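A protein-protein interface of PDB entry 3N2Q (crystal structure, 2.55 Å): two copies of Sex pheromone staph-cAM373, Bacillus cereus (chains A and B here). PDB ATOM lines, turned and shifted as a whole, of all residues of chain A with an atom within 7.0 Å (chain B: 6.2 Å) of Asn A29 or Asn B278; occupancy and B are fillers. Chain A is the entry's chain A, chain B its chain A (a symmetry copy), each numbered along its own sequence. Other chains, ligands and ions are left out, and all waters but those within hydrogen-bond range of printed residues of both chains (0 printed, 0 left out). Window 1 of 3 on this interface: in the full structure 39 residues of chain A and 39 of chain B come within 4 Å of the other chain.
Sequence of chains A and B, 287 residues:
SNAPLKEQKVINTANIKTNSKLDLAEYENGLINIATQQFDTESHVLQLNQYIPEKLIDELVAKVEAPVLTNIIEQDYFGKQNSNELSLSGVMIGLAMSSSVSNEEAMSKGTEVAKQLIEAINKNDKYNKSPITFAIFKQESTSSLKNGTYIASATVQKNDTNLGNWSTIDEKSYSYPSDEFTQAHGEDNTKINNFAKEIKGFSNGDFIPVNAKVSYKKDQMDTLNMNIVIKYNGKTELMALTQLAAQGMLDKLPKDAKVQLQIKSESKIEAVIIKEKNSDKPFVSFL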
ATOM      1  N   ASP A  23       1.364  25.840  20.583  1.00  0.00           N
ATOM      2  CA  ASP A  23      -0.083  25.824  20.877  1.00  0.00           C
ATOM      3  C   ASP A  23      -0.783  24.565  20.361  1.00  0.00           C
ATOM      4  O   ASP A  23      -1.757  24.663  19.615  1.00  0.00           O
ATOM      5  CB  ASP A  23      -0.779  27.035  20.267  1.00  0.00           C
ATOM      6  CG  ASP A  23      -0.506  28.298  21.020  1.00  0.00           C
ATOM      7  OD1 ASP A  23      -0.400  28.227  22.267  1.00  0.00           O
ATOM      8  OD2 ASP A  23      -0.402  29.371  20.370  1.00  0.00           O
ATOM      9  N   LEU A  24      -0.286  23.391  20.738  1.00  0.00           N
ATOM     10  CA  LEU A  24      -0.813  22.132  20.196  1.00  0.00           C
ATOM     11  C   LEU A  24      -2.337  21.963  20.311  1.00  0.00           C
ATOM     12  O   LEU A  24      -2.973  21.503  19.371  1.00  0.00           O
ATOM     13  CB  LEU A  24      -0.086  20.917  20.789  1.00  0.00           C
ATOM     14  CG  LEU A  24      -0.292  19.604  20.012  1.00  0.00           C
ATOM     15  CD1 LEU A  24       0.103  19.730  18.544  1.00  0.00           C
ATOM     16  CD2 LEU A  24       0.450  18.461  20.651  1.00  0.00           C
ATOM     17  N   ALA A  25      -2.914  22.348  21.445  1.00  0.00           N
ATOM     18  CA  ALA A  25      -4.349  22.142  21.677  1.00  0.00           C
ATOM     19  C   ALA A  25      -5.173  22.855  20.610  1.00  0.00           C
ATOM     20  O   ALA A  25      -6.048  22.255  19.981  1.00  0.00           O
ATOM     21  CB  ALA A  25      -4.742  22.603  23.058  1.00  0.00           C
ATOM     22  N   GLU A  26      -4.860  24.127  20.401  1.00  0.00           N
ATOM     23  CA  GLU A  26      -5.502  24.953  19.396  1.00  0.00           C
ATOM     24  C   GLU A  26      -5.271  24.470  17.957  1.00  0.00           C
ATOM     25  O   GLU A  26      -6.164  24.523  17.134  1.00  0.00           O
ATOM     26  CB  GLU A  26      -4.969  26.371  19.523  1.00  0.00           C
ATOM     27  CG  GLU A  26      -6.024  27.407  19.328  1.00  0.00           C
ATOM     28  CD  GLU A  26      -7.048  27.362  20.437  1.00  0.00           C
ATOM     29  OE1 GLU A  26      -8.263  27.280  20.121  1.00  0.00           O
ATOM     30  OE2 GLU A  26      -6.623  27.371  21.623  1.00  0.00           O
ATOM     31  N   TYR A  27      -4.060  24.015  17.675  1.00  0.00           N
ATOM     32  CA  TYR A  27      -3.645  23.595  16.351  1.00  0.00           C
ATOM     33  C   TYR A  27      -4.395  22.331  15.951  1.00  0.00           C
ATOM     34  O   TYR A  27      -4.939  22.260  14.854  1.00  0.00           O
ATOM     35  CB  TYR A  27      -2.125  23.412  16.385  1.00  0.00           C
ATOM     36  CG  TYR A  27      -1.388  22.990  15.122  1.00  0.00           C
ATOM     37  CD1 TYR A  27      -1.787  23.415  13.857  1.00  0.00           C
ATOM     38  CD2 TYR A  27      -0.241  22.194  15.217  1.00  0.00           C
ATOM     39  CE1 TYR A  27      -1.079  23.031  12.702  1.00  0.00           C
ATOM     40  CE2 TYR A  27       0.464  21.796  14.084  1.00  0.00           C
ATOM     41  CZ  TYR A  27       0.046  22.217  12.825  1.00  0.00           C
ATOM     42  OH  TYR A  27       0.759  21.822  11.707  1.00  0.00           O
ATOM     43  N   GLU A  28      -4.456  21.348  16.849  1.00  0.00           N
ATOM     44  CA  GLU A  28      -5.255  20.129  16.642  1.00  0.00           C
ATOM     45  C   GLU A  28      -6.761  20.407  16.606  1.00  0.00           C
ATOM     46  O   GLU A  28      -7.433  20.114  15.608  1.00  0.00           O
ATOM     47  CB  GLU A  28      -4.964  19.097  17.739  1.00  0.00           C
ATOM     48  CG  GLU A  28      -3.711  18.268  17.536  1.00  0.00           C
ATOM     49  CD  GLU A  28      -3.221  17.591  18.822  1.00  0.00           C
ATOM     50  OE1 GLU A  28      -3.758  17.839  19.932  1.00  0.00           O
ATOM     51  OE2 GLU A  28      -2.270  16.799  18.723  1.00  0.00           O
ATOM     52  N   ASN A  29      -7.281  20.971  17.699  1.00  0.00           N
ATOM     53  CA  ASN A  29      -8.724  21.150  17.850  1.00  0.00           C
ATOM     54  C   ASN A  29      -9.346  22.086  16.833  1.00  0.00           C
ATOM     55  O   ASN A  29     -10.439  21.809  16.333  1.00  0.00           O
ATOM     56  CB  ASN A  29      -9.098  21.579  19.264  1.00  0.00           C
ATOM     57  CG  ASN A  29      -9.053  20.425  20.241  1.00  0.00           C
ATOM     58  OD1 ASN A  29      -9.588  19.335  19.975  1.00  0.00           O
ATOM     59  ND2 ASN A  29      -8.421  20.651  21.387  1.00  0.00           N
ATOM     60  N   GLY A  30      -8.654  23.177  16.517  1.00  0.00           N
ATOM     61  CA  GLY A  30      -9.125  24.109  15.511  1.00  0.00           C
ATOM     62  C   GLY A  30      -9.377  23.407  14.186  1.00  0.00           C
ATOM     63  O   GLY A  30     -10.353  23.678  13.512  1.00  0.00           O
ATOM     64  N   LEU A  31      -8.493  22.477  13.836  1.00  0.00           N
ATOM     65  CA  LEU A  31      -8.599  21.723  12.596  1.00  0.00           C
ATOM     66  C   LEU A  31      -9.773  20.769  12.632  1.00  0.00           C
ATOM     67  O   LEU A  31     -10.447  20.568  11.622  1.00  0.00           O
ATOM     68  CB  LEU A  31      -7.297  20.987  12.289  1.00  0.00           C
ATOM     69  CG  LEU A  31      -7.187  20.349  10.910  1.00  0.00           C
ATOM     70  CD1 LEU A  31      -7.307  21.398   9.776  1.00  0.00           C
ATOM     71  CD2 LEU A  31      -5.888  19.550  10.789  1.00  0.00           C
ATOM     72  N   ILE A  32     -10.042  20.199  13.798  1.00  0.00           N
ATOM     73  CA  ILE A  32     -11.223  19.359  13.942  1.00  0.00           C
ATOM     74  C   ILE A  32     -12.474  20.206  13.718  1.00  0.00           C
ATOM     75  O   ILE A  32     -13.423  19.739  13.087  1.00  0.00           O
ATOM     76  CB  ILE A  32     -11.277  18.618  15.300  1.00  0.00           C
ATOM     77  CG1 ILE A  32     -10.200  17.529  15.348  1.00  0.00           C
ATOM     78  CG2 ILE A  32     -12.695  18.013  15.555  1.00  0.00           C
ATOM     79  CD1 ILE A  32      -9.893  17.015  16.752  1.00  0.00           C
ATOM     80  N   ASN A  33     -12.459  21.455  14.189  1.00  0.00           N
ATOM     81  CA  ASN A  33     -13.618  22.323  14.044  1.00  0.00           C
ATOM     82  C   ASN A  33     -13.935  22.666  12.596  1.00  0.00           C
ATOM     83  O   ASN A  33     -15.099  22.740  12.198  1.00  0.00           O
ATOM     84  CB  ASN A  33     -13.463  23.595  14.862  1.00  0.00           C
ATOM     85  CG  ASN A  33     -14.788  24.303  15.058  1.00  0.00           C
ATOM     86  OD1 ASN A  33     -15.294  24.996  14.163  1.00  0.00           O
ATOM     87  ND2 ASN A  33     -15.383  24.097  16.226  1.00  0.00           N
ATOM     88  N   ILE A  34     -12.887  22.872  11.816  1.00  0.00           N
ATOM     89  CA  ILE A  34     -13.020  23.172  10.399  1.00  0.00           C
ATOM     90  C   ILE A  34     -13.644  21.993   9.656  1.00  0.00           C
ATOM     91  O   ILE A  34     -14.477  22.173   8.786  1.00  0.00           O
ATOM     92  CB  ILE A  34     -11.657  23.578   9.794  1.00  0.00           C
ATOM     93  CG1 ILE A  34     -11.244  24.935  10.355  1.00  0.00           C
ATOM     94  CG2 ILE A  34     -11.731  23.628   8.257  1.00  0.00           C
ATOM     95  CD1 ILE A  34      -9.821  25.306  10.117  1.00  0.00           C
ATOM     96  N   ALA A  35     -13.238  20.788  10.028  1.00  0.00           N
ATOM     97  CA  ALA A  35     -13.823  19.562   9.510  1.00  0.00           C
ATOM     98  C   ALA A  35     -15.339  19.523   9.676  1.00  0.00           C
ATOM     99  O   ALA A  35     -16.062  19.261   8.713  1.00  0.00           O
ATOM    100  CB  ALA A  35     -13.182  18.361  10.193  1.00  0.00           C
ATOM    101  N   ILE A  73       0.153  18.890  10.143  1.00  0.00           N
ATOM    102  CA  ILE A  73      -0.628  17.807  10.718  1.00  0.00           C
ATOM    103  C   ILE A  73      -1.687  17.374   9.720  1.00  0.00           C
ATOM    104  O   ILE A  73      -2.213  18.186   8.937  1.00  0.00           O
ATOM    105  CB  ILE A  73      -1.231  18.143  12.092  1.00  0.00           C
ATOM    106  CG1 ILE A  73      -2.369  19.172  11.987  1.00  0.00           C
ATOM    107  CG2 ILE A  73      -0.133  18.575  13.053  1.00  0.00           C
ATOM    108  CD1 ILE A  73      -2.818  19.768  13.334  1.00  0.00           C
ATOM    109  N   GLN A  75      -5.193  15.155   9.308  1.00  0.00           N
ATOM    110  CA  GLN A  75      -6.330  14.473   9.894  1.00  0.00           C
ATOM    111  C   GLN A  75      -7.211  13.842   8.810  1.00  0.00           C
ATOM    112  O   GLN A  75      -7.753  14.537   7.940  1.00  0.00           O
ATOM    113  CB  GLN A  75      -7.126  15.437  10.764  1.00  0.00           C
ATOM    114  CG  GLN A  75      -6.390  15.877  12.022  1.00  0.00           C
ATOM    115  CD  GLN A  75      -7.174  16.912  12.804  1.00  0.00           C
ATOM    116  OE1 GLN A  75      -8.220  17.374  12.355  1.00  0.00           O
ATOM    117  NE2 GLN A  75      -6.672  17.288  13.974  1.00  0.00           N
ATOM    118  N   TYR A 150      -6.585  29.765  13.608  1.00  0.00           N
ATOM    119  CA  TYR A 150      -6.795  29.478  12.192  1.00  0.00           C
ATOM    120  C   TYR A 150      -7.326  30.692  11.444  1.00  0.00           C
ATOM    121  O   TYR A 150      -8.281  31.346  11.887  1.00  0.00           O
ATOM    122  CB  TYR A 150      -7.700  28.266  12.008  1.00  0.00           C
ATOM    123  CG  TYR A 150      -6.923  26.987  12.105  1.00  0.00           C
ATOM    124  CD1 TYR A 150      -6.164  26.526  11.016  1.00  0.00           C
ATOM    125  CD2 TYR A 150      -6.891  26.261  13.288  1.00  0.00           C
ATOM    126  CE1 TYR A 150      -5.416  25.359  11.101  1.00  0.00           C
ATOM    127  CE2 TYR A 150      -6.157  25.081  13.383  1.00  0.00           C
ATOM    128  CZ  TYR A 150      -5.418  24.637  12.290  1.00  0.00           C
ATOM    129  OH  TYR A 150      -4.690  23.462  12.384  1.00  0.00           O
ATOM    130  N   ASP A 256     -15.168  26.531  28.781  1.00  0.00           N
ATOM    131  CA  ASP A 256     -14.696  26.052  27.476  1.00  0.00           C
ATOM    132  C   ASP A 256     -14.428  27.188  26.474  1.00  0.00           C
ATOM    133  O   ASP A 256     -14.247  26.943  25.278  1.00  0.00           O
ATOM    134  CB  ASP A 256     -15.638  24.969  26.895  1.00  0.00           C
ATOM    135  CG  ASP A 256     -17.035  25.496  26.582  1.00  0.00           C
ATOM    136  OD1 ASP A 256     -17.363  26.636  26.976  1.00  0.00           O
ATOM    137  OD2 ASP A 256     -17.816  24.765  25.937  1.00  0.00           O
ATOM    138  N   LYS A 277      -8.225  28.247  26.915  1.00  0.00           N
ATOM    139  CA  LYS A 277      -9.453  27.553  26.496  1.00  0.00           C
ATOM    140  C   LYS A 277     -10.116  26.730  27.609  1.00  0.00           C
ATOM    141  O   LYS A 277     -11.243  27.032  28.003  1.00  0.00           O
ATOM    142  CB  LYS A 277      -9.253  26.723  25.216  1.00  0.00           C
ATOM    143  CG  LYS A 277      -9.315  27.541  23.926  1.00  0.00           C
ATOM    144  CD  LYS A 277     -10.726  27.959  23.578  1.00  0.00           C
ATOM    145  CE  LYS A 277     -10.771  28.639  22.221  1.00  0.00           C
ATOM    146  NZ  LYS A 277     -10.858  27.658  21.103  1.00  0.00           N
ATOM    147  N   ASN A 278      -9.425  25.722  28.124  1.00  0.00           N
ATOM    148  CA  ASN A 278      -9.863  25.052  29.337  1.00  0.00           C
ATOM    149  C   ASN A 278      -8.731  25.185  30.341  1.00  0.00           C
ATOM    150  O   ASN A 278      -7.823  24.360  30.367  1.00  0.00           O
ATOM    151  CB  ASN A 278     -10.151  23.562  29.102  1.00  0.00           C
ATOM    152  CG  ASN A 278     -11.014  23.290  27.865  1.00  0.00           C
ATOM    153  OD1 ASN A 278     -10.510  22.797  26.845  1.00  0.00           O
ATOM    154  ND2 ASN A 278     -12.317  23.571  27.963  1.00  0.00           N
ATOM    155  N   SER A 279      -8.760  26.234  31.151  1.00  0.00           N
ATOM    156  CA  SER A 279      -7.753  26.391  32.182  1.00  0.00           C
ATOM    157  C   SER A 279      -8.383  26.320  33.555  1.00  0.00           C
ATOM    158  O   SER A 279      -9.385  26.961  33.828  1.00  0.00           O
ATOM    159  CB  SER A 279      -6.993  27.698  32.007  1.00  0.00           C
ATOM    160  OG  SER A 279      -6.207  27.975  33.149  1.00  0.00           O
ATOM    161  N   ASP A 280      -7.771  25.528  34.424  1.00  0.00           N
ATOM    162  CA  ASP A 280      -8.242  25.360  35.797  1.00  0.00           C
ATOM    163  C   ASP A 280      -8.279  26.658  36.619  1.00  0.00           C
ATOM    164  O   ASP A 280      -8.945  26.715  37.652  1.00  0.00           O
ATOM    165  CB  ASP A 280      -7.380  24.315  36.502  1.00  0.00           C
ATOM    166  CG  ASP A 280      -7.669  22.890  36.023  1.00  0.00           C
ATOM    167  OD1 ASP A 280      -8.394  22.742  35.017  1.00  0.00           O
ATOM    168  OD2 ASP A 280      -7.164  21.921  36.656  1.00  0.00           O
ATOM    169  N   LYS B 255     -16.603  14.937  28.840  1.00  0.00           N
ATOM    170  CA  LYS B 255     -15.640  15.534  27.916  1.00  0.00           C
ATOM    171  C   LYS B 255     -14.380  16.055  28.609  1.00  0.00           C
ATOM    172  O   LYS B 255     -13.331  16.138  27.981  1.00  0.00           O
ATOM    173  CB  LYS B 255     -16.294  16.653  27.100  1.00  0.00           C
ATOM    174  N   ASP B 256     -14.481  16.407  29.891  1.00  0.00           N
ATOM    175  CA  ASP B 256     -13.333  16.935  30.637  1.00  0.00           C
ATOM    176  C   ASP B 256     -12.445  15.834  31.240  1.00  0.00           C
ATOM    177  O   ASP B 256     -11.579  16.111  32.076  1.00  0.00           O
ATOM    178  CB  ASP B 256     -13.774  17.976  31.695  1.00  0.00           C
ATOM    179  CG  ASP B 256     -14.652  17.381  32.791  1.00  0.00           C
ATOM    180  OD1 ASP B 256     -15.090  16.218  32.662  1.00  0.00           O
ATOM    181  OD2 ASP B 256     -14.908  18.081  33.794  1.00  0.00           O
ATOM    182  N   ALA B 257     -12.667  14.590  30.805  1.00  0.00           N
ATOM    183  CA  ALA B 257     -11.821  13.451  31.181  1.00  0.00           C
ATOM    184  C   ALA B 257     -10.971  12.972  29.998  1.00  0.00           C
ATOM    185  O   ALA B 257     -11.360  13.143  28.842  1.00  0.00           O
ATOM    186  CB  ALA B 257     -12.672  12.332  31.698  1.00  0.00           C
ATOM    187  N   LYS B 258      -9.805  12.397  30.288  1.00  0.00           N
ATOM    188  CA  LYS B 258      -9.034  11.710  29.260  1.00  0.00           C
ATOM    189  C   LYS B 258      -9.548  10.280  29.136  1.00  0.00           C
ATOM    190  O   LYS B 258      -9.514   9.518  30.091  1.00  0.00           O
ATOM    191  CB  LYS B 258      -7.540  11.682  29.577  1.00  0.00           C
ATOM    192  CG  LYS B 258      -6.702  11.153  28.411  1.00  0.00           C
ATOM    193  CD  LYS B 258      -5.404  10.500  28.877  1.00  0.00           C
ATOM    194  CE  LYS B 258      -4.919   9.413  27.876  1.00  0.00           C
ATOM    195  NZ  LYS B 258      -4.370   9.929  26.560  1.00  0.00           N
ATOM    196  N   LYS B 275      -9.428  10.039  23.302  1.00  0.00           N
ATOM    197  CA  LYS B 275     -10.069  11.323  23.399  1.00  0.00           C
ATOM    198  C   LYS B 275      -9.338  12.031  24.526  1.00  0.00           C
ATOM    199  O   LYS B 275      -9.536  11.719  25.699  1.00  0.00           O
ATOM    200  CB  LYS B 275     -11.535  11.133  23.736  1.00  0.00           C
ATOM    201  CG  LYS B 275     -12.376  12.383  23.662  1.00  0.00           C
ATOM    202  CD  LYS B 275     -13.553  12.289  24.622  1.00  0.00           C
ATOM    203  CE  LYS B 275     -13.197  12.865  25.980  1.00  0.00           C
ATOM    204  NZ  LYS B 275     -13.192  14.356  25.905  1.00  0.00           N
ATOM    205  N   GLU B 276      -8.468  12.965  24.169  1.00  0.00           N
ATOM    206  CA  GLU B 276      -7.589  13.597  25.140  1.00  0.00           C
ATOM    207  C   GLU B 276      -8.410  14.537  26.015  1.00  0.00           C
ATOM    208  O   GLU B 276      -9.601  14.728  25.747  1.00  0.00           O
ATOM    209  CB  GLU B 276      -6.432  14.311  24.444  1.00  0.00           C
ATOM    210  CG  GLU B 276      -5.070  13.965  25.028  1.00  0.00           C
ATOM    211  CD  GLU B 276      -3.956  14.005  23.973  1.00  0.00           C
ATOM    212  OE1 GLU B 276      -3.879  13.051  23.167  1.00  0.00           O
ATOM    213  OE2 GLU B 276      -3.161  14.985  23.942  1.00  0.00           O
ATOM    214  N   LYS B 277      -7.782  15.102  27.056  1.00  0.00           N
ATOM    215  CA  LYS B 277      -8.526  15.736  28.155  1.00  0.00           C
ATOM    216  C   LYS B 277      -9.777  16.502  27.701  1.00  0.00           C
ATOM    217  O   LYS B 277     -10.889  16.133  28.079  1.00  0.00           O
ATOM    218  CB  LYS B 277      -7.626  16.599  29.055  1.00  0.00           C
ATOM    219  CG  LYS B 277      -6.837  15.803  30.094  1.00  0.00           C
ATOM    220  CD  LYS B 277      -7.710  15.316  31.229  1.00  0.00           C
ATOM    221  CE  LYS B 277      -6.873  14.660  32.314  1.00  0.00           C
ATOM    222  NZ  LYS B 277      -6.305  15.655  33.266  1.00  0.00           N
ATOM    223  N   ASN B 278      -9.605  17.535  26.888  1.00  0.00           N
ATOM    224  CA  ASN B 278     -10.732  18.158  26.215  1.00  0.00           C
ATOM    225  C   ASN B 278     -10.453  18.067  24.724  1.00  0.00           C
ATOM    226  O   ASN B 278      -9.799  18.940  24.160  1.00  0.00           O
ATOM    227  CB  ASN B 278     -10.894  19.635  26.605  1.00  0.00           C
ATOM    228  CG  ASN B 278     -10.825  19.883  28.116  1.00  0.00           C
ATOM    229  OD1 ASN B 278      -9.828  20.422  28.618  1.00  0.00           O
ATOM    230  ND2 ASN B 278     -11.896  19.530  28.835  1.00  0.00           N
ATOM    231  N   SER B 279     -10.917  17.004  24.085  1.00  0.00           N
ATOM    232  CA  SER B 279     -10.752  16.882  22.650  1.00  0.00           C
ATOM    233  C   SER B 279     -12.097  16.894  21.957  1.00  0.00           C
ATOM    234  O   SER B 279     -13.018  16.195  22.347  1.00  0.00           O
ATOM    235  CB  SER B 279      -9.977  15.621  22.295  1.00  0.00           C
ATOM    236  OG  SER B 279     -10.047  15.366  20.907  1.00  0.00           O
ATOM    237  N   ASP B 280     -12.192  17.702  20.910  1.00  0.00           N
ATOM    238  CA  ASP B 280     -13.418  17.818  20.121  1.00  0.00           C
ATOM    239  C   ASP B 280     -13.882  16.505  19.472  1.00  0.00           C
ATOM    240  O   ASP B 280     -15.039  16.394  19.067  1.00  0.00           O
ATOM    241  CB  ASP B 280     -13.229  18.895  19.055  1.00  0.00           C
ATOM    242  CG  ASP B 280     -13.238  20.311  19.636  1.00  0.00           C
ATOM    243  OD1 ASP B 280     -13.197  20.439  20.878  1.00  0.00           O
ATOM    244  OD2 ASP B 280     -13.283  21.294  18.845  1.00  0.00           O
ATOM    245  N   LYS B 281     -12.976  15.529  19.378  1.00  0.00           N
ATOM    246  CA  LYS B 281     -13.216  14.286  18.642  1.00  0.00           C
ATOM    247  C   LYS B 281     -12.059  13.312  18.880  1.00  0.00           C
ATOM    248  O   LYS B 281     -10.899  13.734  18.858  1.00  0.00           O
ATOM    249  CB  LYS B 281     -13.346  14.567  17.145  1.00  0.00           C
ATOM    250  CG  LYS B 281     -13.470  13.327  16.303  1.00  0.00           C
ATOM    251  CD  LYS B 281     -13.895  13.641  14.897  1.00  0.00           C
ATOM    252  CE  LYS B 281     -14.268  12.364  14.171  1.00  0.00           C
ATOM    253  NZ  LYS B 281     -15.693  11.972  14.367  1.00  0.00           N
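OD1 of Asn A29 is in hydrogen-bond range of N of Asp B280, 3.2 Å away. The side-chain amide oxygen of Asn B278 lies close to the side-chain amide oxygen of Asn A278.
Of the printed residues of chain B, Asn A29 touches Asn B278, Ser B279 and Asp B280. Asn B278 touches just these residues of chain A: Asn A29 (3.5 Å) and Asn A278 (3.0 Å). Of the printed residues of chain B, Asn A278 touches Asn B278. Printed residues of chain A within 4 Å of Asp B280: Asn A29 (3.2 Å) and Ile A32 (3.6 Å). Printed residues of chain A within 4 Å of Lys B281: Ile A32. Leu A24 touches none of the printed residues of chain B. The nearest residue of chain B that does not touch Asn A29 is Lys B281 (5.1 Å). The nearest residue of chain A that does not touch Asn B278 is Ala A25 (6.3 Å). The nearest printed residue of chain A that does not touch Asp B280 is Asn A33 (4.4 Å).
O of Ala A25 lies within hydrogen-bond range of ND2 of Asn A29 (3.2 Å). The side-chain hydroxyl of Ser B279 lies within hydrogen-bond range of the backbone carbonyl oxygen of Lys B281 (2.8 Å).
Among the printed residues, merely in contact across the chains: Asn A29 with Asn B278 (3.5 Å), Asn A29 with Ser B279 (3.8 Å), Ile A32 with Asp B280 (3.6 Å) and Ile A32 with Lys B281 (3.9 Å).
Of the 21 printed residues of chain A, 3 touch a printed residue of chain B. Hydrophobic or aromatic side chains of chain A within 4 Å of the printed part of chain B: Ile A32. Of the 11 printed residues of chain B, 4 touch a printed residue of chain A. Among the printed residues, 6 pairs touch across the chains.
Asn A278 touches its own counterpart, Asn B278. Positions printed for both chains: 256, 277, 278, 279 and 280. Of the 6 pairs that touch across the chains among the printed residues, 1 has its exchanged pair printed and touching as well.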
